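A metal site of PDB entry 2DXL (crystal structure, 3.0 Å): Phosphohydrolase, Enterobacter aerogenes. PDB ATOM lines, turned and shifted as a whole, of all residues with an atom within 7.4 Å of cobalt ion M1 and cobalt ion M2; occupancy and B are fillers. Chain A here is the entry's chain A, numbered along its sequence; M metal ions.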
ATOM      1  N   SER A   7     -13.853   9.598 -10.763  1.00  0.00           N
ATOM      2  CA  SER A   7     -13.035  10.651 -11.312  1.00  0.00           C
ATOM      3  C   SER A   7     -13.497  11.037 -12.688  1.00  0.00           C
ATOM      4  O   SER A   7     -14.182  10.250 -13.368  1.00  0.00           O
ATOM      5  CB  SER A   7     -11.580  10.192 -11.391  1.00  0.00           C
ATOM      6  OG  SER A   7     -10.744  11.223 -11.915  1.00  0.00           O
ATOM      7  N   ASP A   8     -13.130  12.252 -13.104  1.00  0.00           N
ATOM      8  CA  ASP A   8     -13.247  12.648 -14.484  1.00  0.00           C
ATOM      9  C   ASP A   8     -14.643  12.477 -15.028  1.00  0.00           C
ATOM     10  O   ASP A   8     -14.838  11.817 -16.043  1.00  0.00           O
ATOM     11  CB  ASP A   8     -12.262  11.837 -15.310  1.00  0.00           C
ATOM     12  CG  ASP A   8     -10.874  12.408 -15.269  1.00  0.00           C
ATOM     13  OD1 ASP A   8     -10.667  13.441 -15.972  1.00  0.00           O
ATOM     14  OD2 ASP A   8     -10.022  11.840 -14.532  1.00  0.00           O
ATOM     15  N   THR A   9     -15.608  13.076 -14.330  1.00  0.00           N
ATOM     16  CA  THR A   9     -17.013  13.019 -14.698  1.00  0.00           C
ATOM     17  C   THR A   9     -17.326  13.804 -15.965  1.00  0.00           C
ATOM     18  O   THR A   9     -18.222  13.436 -16.716  1.00  0.00           O
ATOM     19  CB  THR A   9     -17.854  13.577 -13.576  1.00  0.00           C
ATOM     20  OG1 THR A   9     -17.361  14.879 -13.246  1.00  0.00           O
ATOM     21  CG2 THR A   9     -17.748  12.693 -12.377  1.00  0.00           C
ATOM     22  N   HIS A  10     -16.574  14.884 -16.191  1.00  0.00           N
ATOM     23  CA  HIS A  10     -16.655  15.711 -17.414  1.00  0.00           C
ATOM     24  C   HIS A  10     -18.063  16.202 -17.777  1.00  0.00           C
ATOM     25  O   HIS A  10     -18.461  16.103 -18.949  1.00  0.00           O
ATOM     26  CB  HIS A  10     -16.030  14.979 -18.606  1.00  0.00           C
ATOM     27  CG  HIS A  10     -14.531  15.004 -18.629  1.00  0.00           C
ATOM     28  ND1 HIS A  10     -13.807  15.814 -19.476  1.00  0.00           N
ATOM     29  CD2 HIS A  10     -13.618  14.315 -17.900  1.00  0.00           C
ATOM     30  CE1 HIS A  10     -12.516  15.618 -19.270  1.00  0.00           C
ATOM     31  NE2 HIS A  10     -12.370  14.718 -18.319  1.00  0.00           N
ATOM     32  N   SER A  48     -12.023  13.003  -7.978  1.00  0.00           N
ATOM     33  CA  SER A  48     -10.685  13.584  -8.190  1.00  0.00           C
ATOM     34  C   SER A  48     -10.555  14.335  -9.518  1.00  0.00           C
ATOM     35  O   SER A  48      -9.476  14.445 -10.087  1.00  0.00           O
ATOM     36  CB  SER A  48      -9.650  12.465  -8.147  1.00  0.00           C
ATOM     37  OG  SER A  48      -9.963  11.487  -9.131  1.00  0.00           O
ATOM     38  N   GLY A  49     -11.666  14.847 -10.022  1.00  0.00           N
ATOM     39  CA  GLY A  49     -11.845  14.791 -11.466  1.00  0.00           C
ATOM     40  C   GLY A  49     -11.633  16.066 -12.201  1.00  0.00           C
ATOM     41  O   GLY A  49     -11.233  17.084 -11.627  1.00  0.00           O
ATOM     42  N   ASP A  50     -11.850  15.964 -13.499  1.00  0.00           N
ATOM     43  CA  ASP A  50     -12.217  17.105 -14.281  1.00  0.00           C
ATOM     44  C   ASP A  50     -13.728  17.046 -14.108  1.00  0.00           C
ATOM     45  O   ASP A  50     -14.396  16.342 -14.875  1.00  0.00           O
ATOM     46  CB  ASP A  50     -11.843  16.864 -15.728  1.00  0.00           C
ATOM     47  CG  ASP A  50     -10.363  16.910 -15.975  1.00  0.00           C
ATOM     48  OD1 ASP A  50      -9.694  17.877 -15.558  1.00  0.00           O
ATOM     49  OD2 ASP A  50      -9.861  15.987 -16.628  1.00  0.00           O
ATOM     50  N   ILE A  51     -14.253  17.721 -13.081  1.00  0.00           N
ATOM     51  CA  ILE A  51     -15.673  17.587 -12.744  1.00  0.00           C
ATOM     52  C   ILE A  51     -16.539  18.012 -13.945  1.00  0.00           C
ATOM     53  O   ILE A  51     -17.518  17.333 -14.247  1.00  0.00           O
ATOM     54  CB  ILE A  51     -16.103  18.313 -11.407  1.00  0.00           C
ATOM     55  CG1 ILE A  51     -15.863  17.447 -10.172  1.00  0.00           C
ATOM     56  CG2 ILE A  51     -17.595  18.483 -11.339  1.00  0.00           C
ATOM     57  CD1 ILE A  51     -14.475  17.317  -9.760  1.00  0.00           C
ATOM     58  N   VAL A  52     -16.157  19.098 -14.622  1.00  0.00           N
ATOM     59  CA  VAL A  52     -16.857  19.550 -15.850  1.00  0.00           C
ATOM     60  C   VAL A  52     -15.920  19.531 -17.056  1.00  0.00           C
ATOM     61  O   VAL A  52     -14.706  19.486 -16.897  1.00  0.00           O
ATOM     62  CB  VAL A  52     -17.473  20.979 -15.719  1.00  0.00           C
ATOM     63  CG1 VAL A  52     -18.405  21.064 -14.507  1.00  0.00           C
ATOM     64  CG2 VAL A  52     -16.399  22.043 -15.665  1.00  0.00           C
ATOM     65  N   ASN A  53     -16.461  19.590 -18.267  1.00  0.00           N
ATOM     66  CA  ASN A  53     -15.633  19.459 -19.463  1.00  0.00           C
ATOM     67  C   ASN A  53     -15.017  20.758 -19.988  1.00  0.00           C
ATOM     68  O   ASN A  53     -13.883  20.764 -20.434  1.00  0.00           O
ATOM     69  CB  ASN A  53     -16.387  18.753 -20.580  1.00  0.00           C
ATOM     70  CG  ASN A  53     -15.509  18.431 -21.777  1.00  0.00           C
ATOM     71  OD1 ASN A  53     -15.690  18.994 -22.861  1.00  0.00           O
ATOM     72  ND2 ASN A  53     -14.548  17.544 -21.582  1.00  0.00           N
ATOM     73  N   GLY A  79      -9.720  19.491 -11.796  1.00  0.00           N
ATOM     74  CA  GLY A  79      -8.744  19.063 -12.787  1.00  0.00           C
ATOM     75  C   GLY A  79      -8.504  20.183 -13.790  1.00  0.00           C
ATOM     76  O   GLY A  79      -9.104  21.249 -13.694  1.00  0.00           O
ATOM     77  N   ASN A  80      -7.614  19.934 -14.749  1.00  0.00           N
ATOM     78  CA  ASN A  80      -7.314  20.912 -15.793  1.00  0.00           C
ATOM     79  C   ASN A  80      -8.525  21.345 -16.637  1.00  0.00           C
ATOM     80  O   ASN A  80      -8.498  22.409 -17.254  1.00  0.00           O
ATOM     81  CB  ASN A  80      -6.189  20.389 -16.701  1.00  0.00           C
ATOM     82  CG  ASN A  80      -6.581  19.131 -17.444  1.00  0.00           C
ATOM     83  OD1 ASN A  80      -7.006  18.125 -16.852  1.00  0.00           O
ATOM     84  ND2 ASN A  80      -6.451  19.178 -18.775  1.00  0.00           N
ATOM     85  N   HIS A  81      -9.586  20.532 -16.657  1.00  0.00           N
ATOM     86  CA  HIS A  81     -10.814  20.894 -17.351  1.00  0.00           C
ATOM     87  C   HIS A  81     -11.721  21.802 -16.526  1.00  0.00           C
ATOM     88  O   HIS A  81     -12.725  22.305 -17.024  1.00  0.00           O
ATOM     89  CB  HIS A  81     -11.582  19.666 -17.796  1.00  0.00           C
ATOM     90  CG  HIS A  81     -11.052  19.060 -19.054  1.00  0.00           C
ATOM     91  ND1 HIS A  81      -9.953  18.220 -19.076  1.00  0.00           N
ATOM     92  CD2 HIS A  81     -11.439  19.212 -20.345  1.00  0.00           C
ATOM     93  CE1 HIS A  81      -9.696  17.872 -20.317  1.00  0.00           C
ATOM     94  NE2 HIS A  81     -10.583  18.454 -21.109  1.00  0.00           N
ATOM     95  N   ASP A  82     -11.345  22.027 -15.278  1.00  0.00           N
ATOM     96  CA  ASP A  82     -12.130  22.827 -14.375  1.00  0.00           C
ATOM     97  C   ASP A  82     -11.692  24.285 -14.365  1.00  0.00           C
ATOM     98  O   ASP A  82     -10.576  24.614 -14.798  1.00  0.00           O
ATOM     99  CB  ASP A  82     -12.026  22.241 -12.972  1.00  0.00           C
ATOM    100  CG  ASP A  82     -12.988  21.110 -12.762  1.00  0.00           C
ATOM    101  OD1 ASP A  82     -14.213  21.385 -12.793  1.00  0.00           O
ATOM    102  OD2 ASP A  82     -12.528  19.960 -12.572  1.00  0.00           O
ATOM    103  N   SER A 127      -2.825  22.027 -19.808  1.00  0.00           N
ATOM    104  CA  SER A 127      -3.355  20.734 -19.381  1.00  0.00           C
ATOM    105  C   SER A 127      -2.418  20.103 -18.358  1.00  0.00           C
ATOM    106  O   SER A 127      -2.842  19.237 -17.582  1.00  0.00           O
ATOM    107  CB  SER A 127      -3.566  19.800 -20.580  1.00  0.00           C
ATOM    108  OG  SER A 127      -4.569  20.310 -21.435  1.00  0.00           O
ATOM    109  N   HIS A 156      -5.500  15.468  -9.027  1.00  0.00           N
ATOM    110  CA  HIS A 156      -5.953  15.118 -10.362  1.00  0.00           C
ATOM    111  C   HIS A 156      -4.825  14.551 -11.231  1.00  0.00           C
ATOM    112  O   HIS A 156      -5.014  13.508 -11.871  1.00  0.00           O
ATOM    113  CB  HIS A 156      -6.616  16.314 -11.050  1.00  0.00           C
ATOM    114  CG  HIS A 156      -7.117  16.029 -12.436  1.00  0.00           C
ATOM    115  ND1 HIS A 156      -8.127  15.135 -12.688  1.00  0.00           N
ATOM    116  CD2 HIS A 156      -6.743  16.520 -13.639  1.00  0.00           C
ATOM    117  CE1 HIS A 156      -8.361  15.094 -13.989  1.00  0.00           C
ATOM    118  NE2 HIS A 156      -7.537  15.926 -14.591  1.00  0.00           N
ATOM    119  N   HIS A 157      -3.676  15.220 -11.228  1.00  0.00           N
ATOM    120  CA  HIS A 157      -2.597  14.846 -12.134  1.00  0.00           C
ATOM    121  C   HIS A 157      -1.671  13.828 -11.496  1.00  0.00           C
ATOM    122  O   HIS A 157      -1.291  13.984 -10.335  1.00  0.00           O
ATOM    123  CB  HIS A 157      -1.778  16.072 -12.531  1.00  0.00           C
ATOM    124  CG  HIS A 157      -2.514  17.039 -13.407  1.00  0.00           C
ATOM    125  ND1 HIS A 157      -3.375  17.993 -12.915  1.00  0.00           N
ATOM    126  CD2 HIS A 157      -2.488  17.222 -14.751  1.00  0.00           C
ATOM    127  CE1 HIS A 157      -3.850  18.708 -13.917  1.00  0.00           C
ATOM    128  NE2 HIS A 157      -3.328  18.267 -15.042  1.00  0.00           N
ATOM    129  N   MET A 167      -0.602  10.753 -22.228  1.00  0.00           N
ATOM    130  CA  MET A 167      -0.846  11.348 -20.917  1.00  0.00           C
ATOM    131  C   MET A 167       0.366  11.896 -20.159  1.00  0.00           C
ATOM    132  O   MET A 167       0.216  12.710 -19.239  1.00  0.00           O
ATOM    133  CB  MET A 167      -1.623  10.356 -20.052  1.00  0.00           C
ATOM    134  CG  MET A 167      -3.078  10.203 -20.432  1.00  0.00           C
ATOM    135  SD  MET A 167      -3.898  11.808 -20.503  1.00  0.00           S
ATOM    136  CE  MET A 167      -3.887  12.136 -22.252  1.00  0.00           C
ATOM    137  N   ILE A 170       1.446  15.633 -20.324  1.00  0.00           N
ATOM    138  CA  ILE A 170       0.520  16.450 -19.536  1.00  0.00           C
ATOM    139  C   ILE A 170       0.294  15.928 -18.103  1.00  0.00           C
ATOM    140  O   ILE A 170      -0.747  16.176 -17.495  1.00  0.00           O
ATOM    141  CB  ILE A 170      -0.798  16.718 -20.302  1.00  0.00           C
ATOM    142  CG1 ILE A 170      -1.486  15.419 -20.739  1.00  0.00           C
ATOM    143  CG2 ILE A 170      -0.514  17.645 -21.491  1.00  0.00           C
ATOM    144  CD1 ILE A 170      -2.916  15.585 -21.267  1.00  0.00           C
ATOM    145  N   GLY A 194      -6.645  11.244 -11.003  1.00  0.00           N
ATOM    146  CA  GLY A 194      -7.494  11.194 -12.183  1.00  0.00           C
ATOM    147  C   GLY A 194      -6.664  11.356 -13.441  1.00  0.00           C
ATOM    148  O   GLY A 194      -5.613  10.706 -13.591  1.00  0.00           O
ATOM    149  N   HIS A 195      -7.137  12.206 -14.351  1.00  0.00           N
ATOM    150  CA  HIS A 195      -6.416  12.612 -15.559  1.00  0.00           C
ATOM    151  C   HIS A 195      -6.259  11.538 -16.636  1.00  0.00           C
ATOM    152  O   HIS A 195      -6.602  11.779 -17.782  1.00  0.00           O
ATOM    153  CB  HIS A 195      -5.050  13.203 -15.203  1.00  0.00           C
ATOM    154  CG  HIS A 195      -4.522  14.182 -16.212  1.00  0.00           C
ATOM    155  ND1 HIS A 195      -5.221  15.306 -16.598  1.00  0.00           N
ATOM    156  CD2 HIS A 195      -3.354  14.217 -16.899  1.00  0.00           C
ATOM    157  CE1 HIS A 195      -4.513  15.990 -17.473  1.00  0.00           C
ATOM    158  NE2 HIS A 195      -3.376  15.348 -17.675  1.00  0.00           N
ATOM    159  N   ASN A 196      -5.758  10.365 -16.268  1.00  0.00           N
ATOM    160  CA  ASN A 196      -5.419   9.329 -17.251  1.00  0.00           C
ATOM    161  C   ASN A 196      -6.588   8.531 -17.832  1.00  0.00           C
ATOM    162  O   ASN A 196      -6.421   7.849 -18.844  1.00  0.00           O
ATOM    163  CB  ASN A 196      -4.361   8.386 -16.682  1.00  0.00           C
ATOM    164  CG  ASN A 196      -2.944   8.812 -17.021  1.00  0.00           C
ATOM    165  OD1 ASN A 196      -2.584   9.993 -16.935  1.00  0.00           O
ATOM    166  ND2 ASN A 196      -2.124   7.851 -17.415  1.00  0.00           N
ATOM    167  N   HIS A 197      -7.749   8.628 -17.202  1.00  0.00           N
ATOM    168  CA  HIS A 197      -8.944   7.835 -17.563  1.00  0.00           C
ATOM    169  C   HIS A 197      -8.583   6.362 -17.786  1.00  0.00           C
ATOM    170  O   HIS A 197      -8.847   5.791 -18.856  1.00  0.00           O
ATOM    171  CB  HIS A 197      -9.624   8.365 -18.817  1.00  0.00           C
ATOM    172  CG  HIS A 197     -10.187   9.746 -18.668  1.00  0.00           C
ATOM    173  ND1 HIS A 197     -11.521  10.024 -18.912  1.00  0.00           N
ATOM    174  CD2 HIS A 197      -9.607  10.919 -18.330  1.00  0.00           C
ATOM    175  CE1 HIS A 197     -11.728  11.318 -18.720  1.00  0.00           C
ATOM    176  NE2 HIS A 197     -10.591  11.881 -18.359  1.00  0.00           N
ATOM    177  N   GLY A 214     -12.229   6.776 -15.879  1.00  0.00           N
ATOM    178  CA  GLY A 214     -13.249   7.819 -15.770  1.00  0.00           C
ATOM    179  C   GLY A 214     -14.615   7.178 -15.557  1.00  0.00           C
ATOM    180  O   GLY A 214     -14.781   5.972 -15.768  1.00  0.00           O
ATOM    181  N   HIS A 217     -16.215   8.066 -20.409  1.00  0.00           N
ATOM    182  CA  HIS A 217     -15.279   7.630 -21.430  1.00  0.00           C
ATOM    183  C   HIS A 217     -13.881   7.393 -20.859  1.00  0.00           C
ATOM    184  O   HIS A 217     -13.500   7.967 -19.838  1.00  0.00           O
ATOM    185  CB  HIS A 217     -15.245   8.655 -22.539  1.00  0.00           C
ATOM    186  CG  HIS A 217     -14.708   9.983 -22.121  1.00  0.00           C
ATOM    187  ND1 HIS A 217     -15.194  10.662 -21.025  1.00  0.00           N
ATOM    188  CD2 HIS A 217     -13.721  10.753 -22.637  1.00  0.00           C
ATOM    189  CE1 HIS A 217     -14.527  11.789 -20.870  1.00  0.00           C
ATOM    190  NE2 HIS A 217     -13.631  11.871 -21.844  1.00  0.00           N
ATOM    191  N   VAL A 219      -9.491   6.608 -21.728  1.00  0.00           N
ATOM    192  CA  VAL A 219      -8.407   6.732 -22.704  1.00  0.00           C
ATOM    193  C   VAL A 219      -7.377   5.589 -22.599  1.00  0.00           C
ATOM    194  O   VAL A 219      -6.879   5.284 -21.508  1.00  0.00           O
ATOM    195  CB  VAL A 219      -7.775   8.196 -22.814  1.00  0.00           C
ATOM    196  CG1 VAL A 219      -8.278   9.128 -21.733  1.00  0.00           C
ATOM    197  CG2 VAL A 219      -6.249   8.163 -22.860  1.00  0.00           C
HETATM  198 CO    CO M   1     -10.256  13.960 -17.873  1.00  0.00          CO
HETATM  199 CO    CO M   2      -7.460  16.020 -16.830  1.00  0.00          CO
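The backbone carbonyl oxygen (O) of His 197 lies within hydrogen-bond range of the backbone NH (N) of Val 219 (3.1 Å). The side-chain carboxylate (OD1) of Asp 50 lies within hydrogen-bond range of the backbone NH (N) of His 81, 2.9 Å away. The backbone carbonyl oxygen (O) of His 156 lies within hydrogen-bond range of the backbone NH (N) of Gly 194 (2.9 Å). OD2 of Asp 8 sits at hydrogen-bond distance from N of His 195. ND2 of Asn 80 lies within hydrogen-bond range of OG of Ser 127 (3.4 Å). ND2 of Asn 53 sits at hydrogen-bond distance from ND1 of His 10 (2.8 Å). O of Ser 48 sits at hydrogen-bond distance from ND1 of His 156 (3.0 Å). OD2 of Asp 8 is in hydrogen-bond range of OG of Ser 7.
Within 4 Å of cobalt ion M1: Asp 8, His 10, Asp 50 and His 197.
Four residues have an atom within 4 Å of cobalt ion M2: Asp 50, Asn 80, His 156 and His 195.
The side-chain carboxylate (OD1) of Asp 8 is bound to cobalt ion M1. NE2 of His 197 binds cobalt ion M1, 2.2 Å away. NE2 of His 10 is bound to cobalt ion M1 (2.3 Å). Cobalt ion M1 is bound by OD2 of Asp 50. Cobalt ion M1 has four donor atoms within binding distance.
Cobalt ion M2 is bound by the side-chain amide oxygen (OD1) of Asn 80, a ring nitrogen (NE2) of His 156, a ring nitrogen (ND1) of His 195 and the side-chain carboxylate (OD2) of Asp 50.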
